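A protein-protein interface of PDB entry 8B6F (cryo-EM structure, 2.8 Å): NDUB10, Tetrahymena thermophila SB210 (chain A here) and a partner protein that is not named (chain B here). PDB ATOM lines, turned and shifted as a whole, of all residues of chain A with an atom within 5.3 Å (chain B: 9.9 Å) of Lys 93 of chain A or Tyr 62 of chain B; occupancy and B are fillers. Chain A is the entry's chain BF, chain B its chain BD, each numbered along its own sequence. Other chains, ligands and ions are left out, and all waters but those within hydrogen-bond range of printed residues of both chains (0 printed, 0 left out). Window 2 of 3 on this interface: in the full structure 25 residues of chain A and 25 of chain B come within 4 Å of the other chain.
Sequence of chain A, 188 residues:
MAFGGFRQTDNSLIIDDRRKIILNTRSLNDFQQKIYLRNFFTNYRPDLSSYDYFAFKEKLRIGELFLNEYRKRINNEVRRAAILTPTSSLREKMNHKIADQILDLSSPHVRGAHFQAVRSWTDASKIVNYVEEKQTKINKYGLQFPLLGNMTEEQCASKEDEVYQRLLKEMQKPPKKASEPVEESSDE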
ATOM      1  N   ALA A  81      18.666 -21.201  24.483  1.00  0.00           N
ATOM      2  CA  ALA A  81      18.898 -22.636  24.402  1.00  0.00           C
ATOM      3  C   ALA A  81      17.612 -23.383  24.083  1.00  0.00           C
ATOM      4  O   ALA A  81      17.610 -24.312  23.267  1.00  0.00           O
ATOM      5  CB  ALA A  81      19.496 -23.144  25.713  1.00  0.00           C
ATOM      6  N   ALA A  82      16.506 -22.995  24.717  1.00  0.00           N
ATOM      7  CA  ALA A  82      15.237 -23.665  24.455  1.00  0.00           C
ATOM      8  C   ALA A  82      14.820 -23.521  22.997  1.00  0.00           C
ATOM      9  O   ALA A  82      14.342 -24.482  22.384  1.00  0.00           O
ATOM     10  CB  ALA A  82      14.157 -23.100  25.377  1.00  0.00           C
ATOM     11  N   THR A  85      17.812 -25.417  20.621  1.00  0.00           N
ATOM     12  CA  THR A  85      18.006 -26.856  20.782  1.00  0.00           C
ATOM     13  C   THR A  85      16.661 -27.558  20.933  1.00  0.00           C
ATOM     14  O   THR A  85      15.816 -27.098  21.709  1.00  0.00           O
ATOM     15  CB  THR A  85      18.874 -27.154  21.997  1.00  0.00           C
ATOM     16  OG1 THR A  85      20.118 -26.453  21.888  1.00  0.00           O
ATOM     17  CG2 THR A  85      19.154 -28.646  22.112  1.00  0.00           C
ATOM     18  N   SER A  89      17.917 -33.797  24.179  1.00  0.00           N
ATOM     19  CA  SER A  89      19.263 -33.347  24.509  1.00  0.00           C
ATOM     20  C   SER A  89      19.256 -31.952  25.126  1.00  0.00           C
ATOM     21  O   SER A  89      20.323 -31.466  25.514  1.00  0.00           O
ATOM     22  CB  SER A  89      20.203 -33.342  23.294  1.00  0.00           C
ATOM     23  OG  SER A  89      19.805 -32.372  22.342  1.00  0.00           O
ATOM     24  N   LEU A  90      18.104 -31.283  25.219  1.00  0.00           N
ATOM     25  CA  LEU A  90      18.076 -29.950  25.810  1.00  0.00           C
ATOM     26  C   LEU A  90      18.468 -29.995  27.282  1.00  0.00           C
ATOM     27  O   LEU A  90      19.316 -29.218  27.734  1.00  0.00           O
ATOM     28  CB  LEU A  90      16.690 -29.328  25.639  1.00  0.00           C
ATOM     29  CG  LEU A  90      16.480 -27.964  26.305  1.00  0.00           C
ATOM     30  CD1 LEU A  90      17.568 -26.980  25.912  1.00  0.00           C
ATOM     31  CD2 LEU A  90      15.114 -27.409  25.946  1.00  0.00           C
ATOM     32  N   ARG A  91      17.859 -30.902  28.052  1.00  0.00           N
ATOM     33  CA  ARG A  91      18.232 -31.029  29.457  1.00  0.00           C
ATOM     34  C   ARG A  91      19.637 -31.589  29.615  1.00  0.00           C
ATOM     35  O   ARG A  91      20.341 -31.233  30.566  1.00  0.00           O
ATOM     36  CB  ARG A  91      17.230 -31.907  30.203  1.00  0.00           C
ATOM     37  CG  ARG A  91      15.931 -31.199  30.535  1.00  0.00           C
ATOM     38  CD  ARG A  91      15.251 -31.821  31.742  1.00  0.00           C
ATOM     39  NE  ARG A  91      14.003 -31.141  32.064  1.00  0.00           N
ATOM     40  CZ  ARG A  91      13.224 -31.446  33.092  1.00  0.00           C
ATOM     41  NH1 ARG A  91      13.541 -32.414  33.936  1.00  0.00           N
ATOM     42  NH2 ARG A  91      12.094 -30.768  33.274  1.00  0.00           N
ATOM     43  N   GLU A  92      20.063 -32.467  28.705  1.00  0.00           N
ATOM     44  CA  GLU A  92      21.428 -32.977  28.770  1.00  0.00           C
ATOM     45  C   GLU A  92      22.433 -31.843  28.637  1.00  0.00           C
ATOM     46  O   GLU A  92      23.427 -31.793  29.368  1.00  0.00           O
ATOM     47  CB  GLU A  92      21.659 -34.023  27.679  1.00  0.00           C
ATOM     48  CG  GLU A  92      20.967 -35.358  27.922  1.00  0.00           C
ATOM     49  CD  GLU A  92      19.463 -35.292  27.729  1.00  0.00           C
ATOM     50  OE1 GLU A  92      18.935 -34.186  27.491  1.00  0.00           O
ATOM     51  OE2 GLU A  92      18.806 -36.351  27.815  1.00  0.00           O
ATOM     52  N   LYS A  93      22.186 -30.919  27.706  1.00  0.00           N
ATOM     53  CA  LYS A  93      23.083 -29.787  27.526  1.00  0.00           C
ATOM     54  C   LYS A  93      22.915 -28.747  28.625  1.00  0.00           C
ATOM     55  O   LYS A  93      23.866 -28.021  28.933  1.00  0.00           O
ATOM     56  CB  LYS A  93      22.847 -29.155  26.155  1.00  0.00           C
ATOM     57  CG  LYS A  93      23.158 -30.088  24.995  1.00  0.00           C
ATOM     58  CD  LYS A  93      22.846 -29.439  23.660  1.00  0.00           C
ATOM     59  CE  LYS A  93      23.180 -30.369  22.507  1.00  0.00           C
ATOM     60  NZ  LYS A  93      22.896 -29.740  21.189  1.00  0.00           N
ATOM     61  N   MET A  94      21.725 -28.654  29.222  1.00  0.00           N
ATOM     62  CA  MET A  94      21.521 -27.713  30.315  1.00  0.00           C
ATOM     63  C   MET A  94      22.156 -28.193  31.611  1.00  0.00           C
ATOM     64  O   MET A  94      22.549 -27.367  32.441  1.00  0.00           O
ATOM     65  CB  MET A  94      20.030 -27.463  30.540  1.00  0.00           C
ATOM     66  CG  MET A  94      19.406 -26.517  29.530  1.00  0.00           C
ATOM     67  SD  MET A  94      17.709 -26.070  29.944  1.00  0.00           S
ATOM     68  CE  MET A  94      17.941 -25.203  31.496  1.00  0.00           C
ATOM     69  N   ASN A  95      22.272 -29.505  31.808  1.00  0.00           N
ATOM     70  CA  ASN A  95      22.913 -30.023  33.010  1.00  0.00           C
ATOM     71  C   ASN A  95      24.416 -29.811  32.897  1.00  0.00           C
ATOM     72  O   ASN A  95      25.195 -30.767  32.840  1.00  0.00           O
ATOM     73  CB  ASN A  95      22.584 -31.502  33.208  1.00  0.00           C
ATOM     74  CG  ASN A  95      21.106 -31.743  33.418  1.00  0.00           C
ATOM     75  OD1 ASN A  95      20.385 -30.866  33.891  1.00  0.00           O
ATOM     76  ND2 ASN A  95      20.645 -32.936  33.064  1.00  0.00           N
ATOM     77  N   HIS A  96      24.813 -28.547  32.867  1.00  0.00           N
ATOM     78  CA  HIS A  96      26.189 -28.129  32.655  1.00  0.00           C
ATOM     79  C   HIS A  96      26.359 -26.807  33.397  1.00  0.00           C
ATOM     80  O   HIS A  96      25.579 -26.489  34.300  1.00  0.00           O
ATOM     81  CB  HIS A  96      26.494 -28.040  31.150  1.00  0.00           C
ATOM     82  CG  HIS A  96      27.842 -28.573  30.773  1.00  0.00           C
ATOM     83  ND1 HIS A  96      28.965 -27.776  30.704  1.00  0.00           N
ATOM     84  CD2 HIS A  96      28.246 -29.820  30.438  1.00  0.00           C
ATOM     85  CE1 HIS A  96      30.003 -28.512  30.347  1.00  0.00           C
ATOM     86  NE2 HIS A  96      29.593 -29.755  30.178  1.00  0.00           N
ATOM     87  N   ILE A  98      25.421 -24.049  32.829  1.00  0.00           N
ATOM     88  CA  ILE A  98      24.253 -23.172  32.802  1.00  0.00           C
ATOM     89  C   ILE A  98      23.328 -23.460  33.982  1.00  0.00           C
ATOM     90  O   ILE A  98      22.881 -22.540  34.675  1.00  0.00           O
ATOM     91  CB  ILE A  98      23.523 -23.297  31.449  1.00  0.00           C
ATOM     92  CG1 ILE A  98      22.381 -22.281  31.369  1.00  0.00           C
ATOM     93  CG2 ILE A  98      22.997 -24.707  31.240  1.00  0.00           C
ATOM     94  CD1 ILE A  98      21.689 -22.232  30.024  1.00  0.00           C
ATOM     95  N   GLN B  59      30.782 -17.279  28.334  1.00  0.00           N
ATOM     96  CA  GLN B  59      31.591 -18.432  27.970  1.00  0.00           C
ATOM     97  C   GLN B  59      30.675 -19.526  27.447  1.00  0.00           C
ATOM     98  O   GLN B  59      29.479 -19.555  27.746  1.00  0.00           O
ATOM     99  CB  GLN B  59      32.412 -18.943  29.159  1.00  0.00           C
ATOM    100  CG  GLN B  59      31.575 -19.348  30.363  1.00  0.00           C
ATOM    101  CD  GLN B  59      32.422 -19.852  31.511  1.00  0.00           C
ATOM    102  OE1 GLN B  59      33.642 -19.940  31.403  1.00  0.00           O
ATOM    103  NE2 GLN B  59      31.775 -20.186  32.621  1.00  0.00           N
ATOM    104  N   ASN B  60      31.251 -20.433  26.660  1.00  0.00           N
ATOM    105  CA  ASN B  60      30.466 -21.510  26.072  1.00  0.00           C
ATOM    106  C   ASN B  60      29.814 -22.354  27.158  1.00  0.00           C
ATOM    107  O   ASN B  60      30.460 -22.743  28.135  1.00  0.00           O
ATOM    108  CB  ASN B  60      31.353 -22.383  25.184  1.00  0.00           C
ATOM    109  CG  ASN B  60      31.802 -21.667  23.928  1.00  0.00           C
ATOM    110  OD1 ASN B  60      31.094 -20.807  23.405  1.00  0.00           O
ATOM    111  ND2 ASN B  60      32.984 -22.019  23.436  1.00  0.00           N
ATOM    112  N   ALA B  61      28.525 -22.640  26.979  1.00  0.00           N
ATOM    113  CA  ALA B  61      27.752 -23.418  27.938  1.00  0.00           C
ATOM    114  C   ALA B  61      27.633 -24.887  27.558  1.00  0.00           C
ATOM    115  O   ALA B  61      27.734 -25.757  28.428  1.00  0.00           O
ATOM    116  CB  ALA B  61      26.350 -22.820  28.086  1.00  0.00           C
ATOM    117  N   TYR B  62      27.417 -25.187  26.281  1.00  0.00           N
ATOM    118  CA  TYR B  62      27.284 -26.570  25.859  1.00  0.00           C
ATOM    119  C   TYR B  62      28.639 -27.273  25.896  1.00  0.00           C
ATOM    120  O   TYR B  62      29.686 -26.629  25.794  1.00  0.00           O
ATOM    121  CB  TYR B  62      26.713 -26.646  24.445  1.00  0.00           C
ATOM    122  CG  TYR B  62      25.269 -26.214  24.316  1.00  0.00           C
ATOM    123  CD1 TYR B  62      24.497 -25.926  25.436  1.00  0.00           C
ATOM    124  CD2 TYR B  62      24.675 -26.103  23.067  1.00  0.00           C
ATOM    125  CE1 TYR B  62      23.180 -25.537  25.314  1.00  0.00           C
ATOM    126  CE2 TYR B  62      23.358 -25.714  22.935  1.00  0.00           C
ATOM    127  CZ  TYR B  62      22.618 -25.430  24.062  1.00  0.00           C
ATOM    128  OH  TYR B  62      21.306 -25.041  23.936  1.00  0.00           O
ATOM    129  N   PRO B  63      28.648 -28.598  26.045  1.00  0.00           N
ATOM    130  CA  PRO B  63      29.915 -29.331  25.966  1.00  0.00           C
ATOM    131  C   PRO B  63      30.519 -29.229  24.573  1.00  0.00           C
ATOM    132  O   PRO B  63      29.811 -29.133  23.569  1.00  0.00           O
ATOM    133  CB  PRO B  63      29.518 -30.772  26.309  1.00  0.00           C
ATOM    134  CG  PRO B  63      28.067 -30.853  26.001  1.00  0.00           C
ATOM    135  CD  PRO B  63      27.506 -29.495  26.293  1.00  0.00           C
ATOM    136  N   GLU B  64      31.846 -29.256  24.523  1.00  0.00           N
ATOM    137  CA  GLU B  64      32.559 -29.054  23.273  1.00  0.00           C
ATOM    138  C   GLU B  64      32.500 -30.303  22.398  1.00  0.00           C
ATOM    139  O   GLU B  64      32.268 -31.419  22.869  1.00  0.00           O
ATOM    140  CB  GLU B  64      34.017 -28.678  23.543  1.00  0.00           C
ATOM    141  CG  GLU B  64      34.176 -27.411  24.369  1.00  0.00           C
ATOM    142  CD  GLU B  64      35.628 -27.021  24.566  1.00  0.00           C
ATOM    143  OE1 GLU B  64      36.510 -27.690  23.987  1.00  0.00           O
ATOM    144  OE2 GLU B  64      35.887 -26.044  25.299  1.00  0.00           O
ATOM    145  N   ILE B  65      32.712 -30.095  21.097  1.00  0.00           N
ATOM    146  CA  ILE B  65      32.815 -31.175  20.128  1.00  0.00           C
ATOM    147  C   ILE B  65      34.087 -30.961  19.322  1.00  0.00           C
ATOM    148  O   ILE B  65      34.669 -29.876  19.311  1.00  0.00           O
ATOM    149  CB  ILE B  65      31.584 -31.262  19.195  1.00  0.00           C
ATOM    150  CG1 ILE B  65      31.415 -29.967  18.395  1.00  0.00           C
ATOM    151  CG2 ILE B  65      30.334 -31.561  20.012  1.00  0.00           C
ATOM    152  CD1 ILE B  65      30.262 -29.995  17.404  1.00  0.00           C
ATOM    153  N   HIS B  69      34.711 -34.493  14.428  1.00  0.00           N
ATOM    154  CA  HIS B  69      33.274 -34.731  14.480  1.00  0.00           C
ATOM    155  C   HIS B  69      32.527 -33.753  13.582  1.00  0.00           C
ATOM    156  O   HIS B  69      31.554 -34.130  12.918  1.00  0.00           O
ATOM    157  CB  HIS B  69      32.780 -34.625  15.921  1.00  0.00           C
ATOM    158  CG  HIS B  69      31.370 -35.087  16.111  1.00  0.00           C
ATOM    159  ND1 HIS B  69      30.906 -36.285  15.610  1.00  0.00           N
ATOM    160  CD2 HIS B  69      30.324 -34.516  16.751  1.00  0.00           C
ATOM    161  CE1 HIS B  69      29.633 -36.430  15.933  1.00  0.00           C
ATOM    162  NE2 HIS B  69      29.256 -35.371  16.625  1.00  0.00           N
ATOM    163  N   ARG B  70      32.964 -32.493  13.546  1.00  0.00           N
ATOM    164  CA  ARG B  70      32.344 -31.525  12.646  1.00  0.00           C
ATOM    165  C   ARG B  70      32.492 -31.958  11.194  1.00  0.00           C
ATOM    166  O   ARG B  70      31.536 -31.883  10.414  1.00  0.00           O
ATOM    167  CB  ARG B  70      32.960 -30.142  12.848  1.00  0.00           C
ATOM    168  CG  ARG B  70      32.609 -29.486  14.168  1.00  0.00           C
ATOM    169  CD  ARG B  70      33.145 -28.066  14.222  1.00  0.00           C
ATOM    170  NE  ARG B  70      32.751 -27.383  15.447  1.00  0.00           N
ATOM    171  CZ  ARG B  70      33.417 -27.444  16.591  1.00  0.00           C
ATOM    172  NH1 ARG B  70      34.526 -28.155  16.710  1.00  0.00           N
ATOM    173  NH2 ARG B  70      32.956 -26.779  17.645  1.00  0.00           N
ATOM    174  N   LEU B  73      30.116 -34.804  10.467  1.00  0.00           N
ATOM    175  CA  LEU B  73      28.760 -34.317  10.235  1.00  0.00           C
ATOM    176  C   LEU B  73      28.640 -33.671   8.862  1.00  0.00           C
ATOM    177  O   LEU B  73      27.638 -33.858   8.163  1.00  0.00           O
ATOM    178  CB  LEU B  73      28.360 -33.328  11.328  1.00  0.00           C
ATOM    179  CG  LEU B  73      28.295 -33.883  12.754  1.00  0.00           C
ATOM    180  CD1 LEU B  73      27.972 -32.767  13.730  1.00  0.00           C
ATOM    181  CD2 LEU B  73      27.282 -35.010  12.873  1.00  0.00           C
ATOM    182  N   VAL B 150      17.448 -13.931  20.879  1.00  0.00           N
ATOM    183  CA  VAL B 150      17.855 -15.142  20.181  1.00  0.00           C
ATOM    184  C   VAL B 150      18.224 -14.757  18.757  1.00  0.00           C
ATOM    185  O   VAL B 150      17.366 -14.357  17.964  1.00  0.00           O
ATOM    186  CB  VAL B 150      16.753 -16.212  20.221  1.00  0.00           C
ATOM    187  CG1 VAL B 150      17.227 -17.501  19.572  1.00  0.00           C
ATOM    188  CG2 VAL B 150      16.344 -16.452  21.654  1.00  0.00           C
ATOM    189  N   ARG B 153      25.027 -12.891  17.905  1.00  0.00           N
ATOM    190  CA  ARG B 153      25.631 -12.215  19.042  1.00  0.00           C
ATOM    191  C   ARG B 153      26.320 -10.933  18.596  1.00  0.00           C
ATOM    192  O   ARG B 153      26.888 -10.854  17.504  1.00  0.00           O
ATOM    193  CB  ARG B 153      26.651 -13.122  19.736  1.00  0.00           C
ATOM    194  CG  ARG B 153      26.061 -14.359  20.388  1.00  0.00           C
ATOM    195  CD  ARG B 153      25.072 -13.995  21.481  1.00  0.00           C
ATOM    196  NE  ARG B 153      24.594 -15.172  22.196  1.00  0.00           N
ATOM    197  CZ  ARG B 153      25.162 -15.683  23.279  1.00  0.00           C
ATOM    198  NH1 ARG B 153      26.249 -15.148  23.809  1.00  0.00           N
ATOM    199  NH2 ARG B 153      24.624 -16.757  23.847  1.00  0.00           N
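Of the 12 printed residues of chain A, 4 touch a printed residue of chain B.
Of the 12 printed residues of chain B, 2 touch a printed residue of chain A.
Among the printed residues, 4 pairs touch across the chains.
Among the printed residues, no Asp or Glu carboxylate lies within 4 Å of a Lys or Arg side-chain nitrogen of the other chain.
Ala 81 of chain A touches Tyr 62 of chain B.
CD1 of Tyr 62 of chain B touches CB of Lys 93 of chain A, at 3.7 Å.
The side-chain hydroxyl of Thr 85 of chain A lies within hydrogen-bond range of the side-chain hydroxyl of Tyr 62 of chain B (2.8 Å).
The backbone carbonyl oxygen (O) of Ala 61 of chain B lies within hydrogen-bond range of a ring nitrogen (ND1) of His 96 of chain A.
Lys 93 of chain A touches just one residue of chain B: Tyr 62 (3.7 Å).
Of the printed residues of chain B, His 96 of chain A touches Ala 61.
Of the printed residues of chain B, Thr 85 of chain A touches Tyr 62 (2.8 Å).
Printed residues of chain A within 4 Å of Ala 61 of chain B: His 96.
The nearest residue of chain B that does not touch Lys 93 of chain A is Ala 61 of chain B (4.5 Å).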
